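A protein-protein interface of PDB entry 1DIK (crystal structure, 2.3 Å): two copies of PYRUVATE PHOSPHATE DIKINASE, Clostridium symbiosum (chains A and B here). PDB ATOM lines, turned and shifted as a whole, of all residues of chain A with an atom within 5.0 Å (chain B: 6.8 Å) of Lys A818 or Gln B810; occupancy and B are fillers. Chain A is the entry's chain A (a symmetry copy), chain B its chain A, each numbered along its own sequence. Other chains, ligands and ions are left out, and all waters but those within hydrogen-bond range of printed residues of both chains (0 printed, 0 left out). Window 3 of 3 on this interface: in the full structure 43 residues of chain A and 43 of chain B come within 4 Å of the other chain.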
ATOM      1  N   ALA A 750     -23.506  10.980 -28.761  1.00  0.00           N
ATOM      2  CA  ALA A 750     -23.961  10.241 -27.588  1.00  0.00           C
ATOM      3  C   ALA A 750     -23.788   8.711 -27.707  1.00  0.00           C
ATOM      4  O   ALA A 750     -23.450   8.024 -26.740  1.00  0.00           O
ATOM      5  CB  ALA A 750     -25.467  10.576 -27.321  1.00  0.00           C
ATOM      6  N   LEU A 751     -24.116   8.175 -28.874  1.00  0.00           N
ATOM      7  CA  LEU A 751     -24.015   6.734 -29.177  1.00  0.00           C
ATOM      8  C   LEU A 751     -22.622   6.252 -29.138  1.00  0.00           C
ATOM      9  O   LEU A 751     -22.346   5.138 -28.738  1.00  0.00           O
ATOM     10  CB  LEU A 751     -24.596   6.447 -30.590  1.00  0.00           C
ATOM     11  CG  LEU A 751     -26.138   6.597 -30.632  1.00  0.00           C
ATOM     12  CD1 LEU A 751     -26.646   6.765 -32.042  1.00  0.00           C
ATOM     13  CD2 LEU A 751     -26.814   5.445 -29.928  1.00  0.00           C
ATOM     14  N   THR A 752     -21.728   7.113 -29.588  1.00  0.00           N
ATOM     15  CA  THR A 752     -20.313   6.783 -29.614  1.00  0.00           C
ATOM     16  C   THR A 752     -19.540   7.632 -28.618  1.00  0.00           C
ATOM     17  O   THR A 752     -18.388   7.898 -28.837  1.00  0.00           O
ATOM     18  CB  THR A 752     -19.730   6.974 -30.999  1.00  0.00           C
ATOM     19  OG1 THR A 752     -19.601   8.360 -31.271  1.00  0.00           O
ATOM     20  CG2 THR A 752     -20.680   6.374 -32.037  1.00  0.00           C
ATOM     21  N   ALA A 753     -20.192   8.028 -27.525  1.00  0.00           N
ATOM     22  CA  ALA A 753     -19.597   8.837 -26.491  1.00  0.00           C
ATOM     23  C   ALA A 753     -18.347   8.217 -25.831  1.00  0.00           C
ATOM     24  O   ALA A 753     -17.554   8.934 -25.269  1.00  0.00           O
ATOM     25  CB  ALA A 753     -20.609   9.148 -25.472  1.00  0.00           C
ATOM     26  N   ASP A 754     -18.162   6.901 -25.876  1.00  0.00           N
ATOM     27  CA  ASP A 754     -16.989   6.299 -25.244  1.00  0.00           C
ATOM     28  C   ASP A 754     -15.752   6.500 -26.087  1.00  0.00           C
ATOM     29  O   ASP A 754     -14.663   6.581 -25.548  1.00  0.00           O
ATOM     30  CB  ASP A 754     -17.193   4.835 -24.829  1.00  0.00           C
ATOM     31  CG  ASP A 754     -17.539   3.900 -25.991  1.00  0.00           C
ATOM     32  OD1 ASP A 754     -18.243   4.291 -26.910  1.00  0.00           O
ATOM     33  OD2 ASP A 754     -17.115   2.735 -25.989  1.00  0.00           O
ATOM     34  N   MET A 814     -26.754   7.993 -21.881  1.00  0.00           N
ATOM     35  CA  MET A 814     -25.835   6.954 -22.357  1.00  0.00           C
ATOM     36  C   MET A 814     -24.485   7.556 -22.685  1.00  0.00           C
ATOM     37  O   MET A 814     -23.502   6.855 -22.668  1.00  0.00           O
ATOM     38  CB  MET A 814     -26.388   6.145 -23.558  1.00  0.00           C
ATOM     39  CG  MET A 814     -26.125   6.704 -24.963  1.00  0.00           C
ATOM     40  SD  MET A 814     -26.431   5.381 -26.145  1.00  0.00           S
ATOM     41  CE  MET A 814     -28.317   5.055 -25.802  1.00  0.00           C
ATOM     42  N   ALA A 815     -24.482   8.847 -23.003  1.00  0.00           N
ATOM     43  CA  ALA A 815     -23.290   9.604 -23.296  1.00  0.00           C
ATOM     44  C   ALA A 815     -22.501   9.779 -22.009  1.00  0.00           C
ATOM     45  O   ALA A 815     -21.282   9.758 -21.976  1.00  0.00           O
ATOM     46  CB  ALA A 815     -23.679  10.930 -23.813  1.00  0.00           C
ATOM     47  N   VAL A 816     -23.215  10.062 -20.947  1.00  0.00           N
ATOM     48  CA  VAL A 816     -22.565  10.176 -19.685  1.00  0.00           C
ATOM     49  C   VAL A 816     -21.964   8.816 -19.228  1.00  0.00           C
ATOM     50  O   VAL A 816     -20.770   8.721 -18.966  1.00  0.00           O
ATOM     51  CB  VAL A 816     -23.536  10.737 -18.679  1.00  0.00           C
ATOM     52  CG1 VAL A 816     -22.950  10.666 -17.291  1.00  0.00           C
ATOM     53  CG2 VAL A 816     -23.837  12.152 -19.053  1.00  0.00           C
ATOM     54  N   LYS A 817     -22.757   7.751 -19.233  1.00  0.00           N
ATOM     55  CA  LYS A 817     -22.291   6.446 -18.803  1.00  0.00           C
ATOM     56  C   LYS A 817     -21.165   5.920 -19.644  1.00  0.00           C
ATOM     57  O   LYS A 817     -20.295   5.268 -19.132  1.00  0.00           O
ATOM     58  CB  LYS A 817     -23.453   5.449 -18.784  1.00  0.00           C
ATOM     59  CG  LYS A 817     -23.077   4.000 -19.095  1.00  0.00           C
ATOM     60  CD  LYS A 817     -23.116   3.036 -17.902  1.00  0.00           C
ATOM     61  CE  LYS A 817     -24.564   2.673 -17.558  1.00  0.00           C
ATOM     62  NZ  LYS A 817     -24.804   2.076 -16.179  1.00  0.00           N
ATOM     63  N   LYS A 818     -21.258   6.093 -20.953  1.00  0.00           N
ATOM     64  CA  LYS A 818     -20.232   5.631 -21.887  1.00  0.00           C
ATOM     65  C   LYS A 818     -19.031   6.552 -21.931  1.00  0.00           C
ATOM     66  O   LYS A 818     -17.946   6.101 -22.210  1.00  0.00           O
ATOM     67  CB  LYS A 818     -20.788   5.525 -23.295  1.00  0.00           C
ATOM     68  CG  LYS A 818     -21.891   4.512 -23.490  1.00  0.00           C
ATOM     69  CD  LYS A 818     -22.477   4.714 -24.927  1.00  0.00           C
ATOM     70  CE  LYS A 818     -22.771   3.360 -25.636  1.00  0.00           C
ATOM     71  NZ  LYS A 818     -22.781   3.474 -27.152  1.00  0.00           N
ATOM     72  N   GLY A 819     -19.245   7.852 -21.843  1.00  0.00           N
ATOM     73  CA  GLY A 819     -18.117   8.760 -21.820  1.00  0.00           C
ATOM     74  C   GLY A 819     -17.254   8.449 -20.610  1.00  0.00           C
ATOM     75  O   GLY A 819     -16.045   8.350 -20.710  1.00  0.00           O
ATOM     76  N   ARG A 820     -17.905   8.233 -19.476  1.00  0.00           N
ATOM     77  CA  ARG A 820     -17.247   7.895 -18.234  1.00  0.00           C
ATOM     78  C   ARG A 820     -16.690   6.491 -18.129  1.00  0.00           C
ATOM     79  O   ARG A 820     -16.122   6.107 -17.105  1.00  0.00           O
ATOM     80  CB  ARG A 820     -18.120   8.236 -17.039  1.00  0.00           C
ATOM     81  CG  ARG A 820     -18.376   9.695 -16.982  1.00  0.00           C
ATOM     82  CD  ARG A 820     -18.869  10.099 -15.666  1.00  0.00           C
ATOM     83  NE  ARG A 820     -19.000  11.560 -15.556  1.00  0.00           N
ATOM     84  CZ  ARG A 820     -20.060  12.134 -14.990  1.00  0.00           C
ATOM     85  NH1 ARG A 820     -21.002  11.350 -14.535  1.00  0.00           N
ATOM     86  NH2 ARG A 820     -20.171  13.451 -14.845  1.00  0.00           N
ATOM     87  N   GLN A 821     -16.861   5.701 -19.176  1.00  0.00           N
ATOM     88  CA  GLN A 821     -16.241   4.374 -19.193  1.00  0.00           C
ATOM     89  C   GLN A 821     -14.817   4.623 -19.662  1.00  0.00           C
ATOM     90  O   GLN A 821     -13.884   3.947 -19.222  1.00  0.00           O
ATOM     91  CB  GLN A 821     -16.882   3.451 -20.211  1.00  0.00           C
ATOM     92  CG  GLN A 821     -18.316   3.212 -19.920  1.00  0.00           C
ATOM     93  CD  GLN A 821     -18.874   2.056 -20.661  1.00  0.00           C
ATOM     94  OE1 GLN A 821     -18.747   1.932 -21.882  1.00  0.00           O
ATOM     95  NE2 GLN A 821     -19.498   1.182 -19.922  1.00  0.00           N
ATOM     96  N   THR A 822     -14.657   5.551 -20.606  1.00  0.00           N
ATOM     97  CA  THR A 822     -13.346   5.843 -21.113  1.00  0.00           C
ATOM     98  C   THR A 822     -12.657   6.952 -20.315  1.00  0.00           C
ATOM     99  O   THR A 822     -11.450   6.884 -20.028  1.00  0.00           O
ATOM    100  CB  THR A 822     -13.373   6.083 -22.641  1.00  0.00           C
ATOM    101  OG1 THR A 822     -14.036   7.275 -22.953  1.00  0.00           O
ATOM    102  CG2 THR A 822     -14.132   5.030 -23.289  1.00  0.00           C
ATOM    103  N   ALA B 750     -36.468   4.795 -32.544  1.00  0.00           N
ATOM    104  CA  ALA B 750     -35.617   3.704 -32.085  1.00  0.00           C
ATOM    105  C   ALA B 750     -35.445   3.647 -30.551  1.00  0.00           C
ATOM    106  O   ALA B 750     -35.402   2.572 -29.948  1.00  0.00           O
ATOM    107  CB  ALA B 750     -34.210   3.828 -32.762  1.00  0.00           C
ATOM    108  N   ASP B 804     -23.552   2.686 -41.139  1.00  0.00           N
ATOM    109  CA  ASP B 804     -22.650   2.970 -40.057  1.00  0.00           C
ATOM    110  C   ASP B 804     -23.055   2.062 -38.926  1.00  0.00           C
ATOM    111  O   ASP B 804     -24.021   2.335 -38.237  1.00  0.00           O
ATOM    112  CB  ASP B 804     -22.777   4.423 -39.606  1.00  0.00           C
ATOM    113  CG  ASP B 804     -22.132   4.634 -38.281  1.00  0.00           C
ATOM    114  OD1 ASP B 804     -21.084   4.030 -38.035  1.00  0.00           O
ATOM    115  OD2 ASP B 804     -22.709   5.301 -37.441  1.00  0.00           O
ATOM    116  N   GLN B 805     -22.337   0.990 -38.703  1.00  0.00           N
ATOM    117  CA  GLN B 805     -22.721   0.090 -37.622  1.00  0.00           C
ATOM    118  C   GLN B 805     -22.429   0.512 -36.222  1.00  0.00           C
ATOM    119  O   GLN B 805     -22.959  -0.044 -35.298  1.00  0.00           O
ATOM    120  CB  GLN B 805     -22.125  -1.284 -37.842  1.00  0.00           C
ATOM    121  CG  GLN B 805     -22.268  -1.747 -39.285  1.00  0.00           C
ATOM    122  CD  GLN B 805     -21.907  -3.184 -39.465  1.00  0.00           C
ATOM    123  OE1 GLN B 805     -21.548  -3.861 -38.513  1.00  0.00           O
ATOM    124  NE2 GLN B 805     -22.050  -3.680 -40.673  1.00  0.00           N
ATOM    125  N   THR B 806     -21.467   1.385 -36.037  1.00  0.00           N
ATOM    126  CA  THR B 806     -21.135   1.815 -34.679  1.00  0.00           C
ATOM    127  C   THR B 806     -22.129   2.793 -34.104  1.00  0.00           C
ATOM    128  O   THR B 806     -22.405   2.710 -32.943  1.00  0.00           O
ATOM    129  CB  THR B 806     -19.755   2.465 -34.666  1.00  0.00           C
ATOM    130  OG1 THR B 806     -18.835   1.552 -35.273  1.00  0.00           O
ATOM    131  CG2 THR B 806     -19.311   2.827 -33.230  1.00  0.00           C
ATOM    132  N   GLY B 807     -22.620   3.725 -34.920  1.00  0.00           N
ATOM    133  CA  GLY B 807     -23.576   4.727 -34.484  1.00  0.00           C
ATOM    134  C   GLY B 807     -25.008   4.409 -34.877  1.00  0.00           C
ATOM    135  O   GLY B 807     -25.777   3.991 -34.038  1.00  0.00           O
ATOM    136  N   VAL B 808     -25.376   4.644 -36.136  1.00  0.00           N
ATOM    137  CA  VAL B 808     -26.703   4.314 -36.624  1.00  0.00           C
ATOM    138  C   VAL B 808     -27.030   2.854 -36.352  1.00  0.00           C
ATOM    139  O   VAL B 808     -28.160   2.526 -36.068  1.00  0.00           O
ATOM    140  CB  VAL B 808     -26.820   4.479 -38.126  1.00  0.00           C
ATOM    141  CG1 VAL B 808     -28.224   4.076 -38.509  1.00  0.00           C
ATOM    142  CG2 VAL B 808     -26.543   5.915 -38.554  1.00  0.00           C
ATOM    143  N   GLY B 809     -26.043   1.984 -36.443  1.00  0.00           N
ATOM    144  CA  GLY B 809     -26.245   0.572 -36.197  1.00  0.00           C
ATOM    145  C   GLY B 809     -26.777   0.217 -34.847  1.00  0.00           C
ATOM    146  O   GLY B 809     -27.482  -0.787 -34.681  1.00  0.00           O
ATOM    147  N   GLN B 810     -26.373   0.982 -33.845  1.00  0.00           N
ATOM    148  CA  GLN B 810     -26.840   0.782 -32.479  1.00  0.00           C
ATOM    149  C   GLN B 810     -28.368   1.096 -32.293  1.00  0.00           C
ATOM    150  O   GLN B 810     -29.046   0.478 -31.479  1.00  0.00           O
ATOM    151  CB  GLN B 810     -26.078   1.736 -31.562  1.00  0.00           C
ATOM    152  CG  GLN B 810     -24.859   1.141 -30.814  1.00  0.00           C
ATOM    153  CD  GLN B 810     -24.311   2.135 -29.796  1.00  0.00           C
ATOM    154  OE1 GLN B 810     -24.855   2.246 -28.690  1.00  0.00           O
ATOM    155  NE2 GLN B 810     -23.331   2.952 -30.208  1.00  0.00           N
ATOM    156  N   LEU B 811     -28.852   2.112 -32.995  1.00  0.00           N
ATOM    157  CA  LEU B 811     -30.225   2.593 -32.940  1.00  0.00           C
ATOM    158  C   LEU B 811     -31.110   1.562 -33.581  1.00  0.00           C
ATOM    159  O   LEU B 811     -32.247   1.346 -33.150  1.00  0.00           O
ATOM    160  CB  LEU B 811     -30.343   3.911 -33.710  1.00  0.00           C
ATOM    161  CG  LEU B 811     -29.866   5.253 -33.127  1.00  0.00           C
ATOM    162  CD1 LEU B 811     -30.475   6.350 -33.945  1.00  0.00           C
ATOM    163  CD2 LEU B 811     -30.356   5.484 -31.717  1.00  0.00           C
ATOM    164  N   VAL B 812     -30.612   0.972 -34.663  1.00  0.00           N
ATOM    165  CA  VAL B 812     -31.356  -0.077 -35.361  1.00  0.00           C
ATOM    166  C   VAL B 812     -31.418  -1.258 -34.440  1.00  0.00           C
ATOM    167  O   VAL B 812     -32.455  -1.853 -34.233  1.00  0.00           O
ATOM    168  CB  VAL B 812     -30.651  -0.519 -36.634  1.00  0.00           C
ATOM    169  CG1 VAL B 812     -31.178  -1.883 -37.087  1.00  0.00           C
ATOM    170  CG2 VAL B 812     -30.849   0.537 -37.694  1.00  0.00           C
ATOM    171  N   GLU B 813     -30.278  -1.624 -33.903  1.00  0.00           N
ATOM    172  CA  GLU B 813     -30.230  -2.744 -33.022  1.00  0.00           C
ATOM    173  C   GLU B 813     -30.968  -2.574 -31.711  1.00  0.00           C
ATOM    174  O   GLU B 813     -31.347  -3.562 -31.098  1.00  0.00           O
ATOM    175  CB  GLU B 813     -28.805  -3.163 -32.814  1.00  0.00           C
ATOM    176  CG  GLU B 813     -28.565  -4.069 -31.632  1.00  0.00           C
ATOM    177  CD  GLU B 813     -27.381  -4.981 -31.874  1.00  0.00           C
ATOM    178  OE1 GLU B 813     -26.402  -4.500 -32.497  1.00  0.00           O
ATOM    179  OE2 GLU B 813     -27.460  -6.171 -31.476  1.00  0.00           O
ATOM    180  N   MET B 814     -31.239  -1.356 -31.276  1.00  0.00           N
ATOM    181  CA  MET B 814     -31.966  -1.201 -30.012  1.00  0.00           C
ATOM    182  C   MET B 814     -33.458  -1.149 -30.267  1.00  0.00           C
ATOM    183  O   MET B 814     -34.223  -1.458 -29.384  1.00  0.00           O
ATOM    184  CB  MET B 814     -31.503   0.022 -29.180  1.00  0.00           C
ATOM    185  CG  MET B 814     -32.180   1.369 -29.474  1.00  0.00           C
ATOM    186  SD  MET B 814     -31.826   2.472 -28.096  1.00  0.00           S
ATOM    187  CE  MET B 814     -29.887   2.556 -28.224  1.00  0.00           C
ATOM    188  N   ALA B 815     -33.831  -0.732 -31.472  1.00  0.00           N
ATOM    189  CA  ALA B 815     -35.203  -0.664 -31.915  1.00  0.00           C
ATOM    190  C   ALA B 815     -35.722  -2.081 -32.094  1.00  0.00           C
ATOM    191  O   ALA B 815     -36.867  -2.402 -31.823  1.00  0.00           O
ATOM    192  CB  ALA B 815     -35.254   0.042 -33.210  1.00  0.00           C
ATOM    193  N   PHE B 843     -25.151  -7.095 -41.105  1.00  0.00           N
ATOM    194  CA  PHE B 843     -25.453  -6.489 -39.840  1.00  0.00           C
ATOM    195  C   PHE B 843     -26.907  -6.800 -39.548  1.00  0.00           C
ATOM    196  O   PHE B 843     -27.232  -7.269 -38.465  1.00  0.00           O
ATOM    197  CB  PHE B 843     -25.291  -4.970 -39.951  1.00  0.00           C
ATOM    198  CG  PHE B 843     -25.644  -4.248 -38.680  1.00  0.00           C
ATOM    199  CD1 PHE B 843     -24.825  -4.368 -37.554  1.00  0.00           C
ATOM    200  CD2 PHE B 843     -26.825  -3.503 -38.584  1.00  0.00           C
ATOM    201  CE1 PHE B 843     -25.172  -3.768 -36.359  1.00  0.00           C
ATOM    202  CE2 PHE B 843     -27.186  -2.890 -37.381  1.00  0.00           C
ATOM    203  CZ  PHE B 843     -26.359  -3.026 -36.272  1.00  0.00           C
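Of the 14 printed residues of chain B, 5 touch a printed residue of chain A.
Of the 14 printed residues of chain A, 4 touch a printed residue of chain B.
Printed residues of chain A that touch a printed residue of chain B: Leu A751, Thr A752, Met A814 and Lys A818.
Hydrophobic or aromatic side chains of chain A within 4 Å of the printed part of chain B: Leu A751 and Met A814.
Among the printed residues, no Asp or Glu carboxylate lies within 4 Å of a Lys or Arg side-chain nitrogen of the other chain.
Met B814 touches its own counterpart, Met A814.
Of the 6 pairs that touch across the chains among the printed residues, 1 has its exchanged pair printed and touching as well.
Among the printed residues, pairs that only touch across the chains: Leu A751 with Gly B807, Leu A751 with Leu B811, Met A814 with Met B814 and Thr A752 with Thr B806.
The backbone NH of Thr B806 is in hydrogen-bond range of the side-chain carboxylate of Asp B804, 3.3 Å away.
The side-chain carboxylate (OD2) of Asp B804 is in hydrogen-bond range of the backbone NH (N) of Gly B807 (3.0 Å).
The backbone carbonyl oxygen (O) of Thr B806 lies within hydrogen-bond range of the side-chain amide nitrogen (NE2) of Gln B810 (2.9 Å).
Of chain B, only Gln B810 comes within 4 Å of Lys A818.
Printed residues of chain A within 4 Å of Thr B806: Thr A752 (3.98 Å).
Of the printed residues of chain A, Gly B807 touches Leu A751 (3.5 Å).
Of the printed residues of chain A, Leu B811 touches Leu A751 (3.7 Å).
The nearest residue of chain B that does not touch Lys A818 is Thr B806 (5.9 Å).
The nearest residue of chain A that does not touch Gln B810 is Met A814 (4.3 Å).
The nearest printed residue of chain A that does not touch Thr B806 is Leu A751 (4.9 Å).
The side-chain amide nitrogen of Gln B810 lies within hydrogen-bond range of the backbone carbonyl oxygen of Leu A751, at 2.8 Å.
NZ of Lys A818 is in hydrogen-bond range of OE1 of Gln B810 (2.9 Å).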
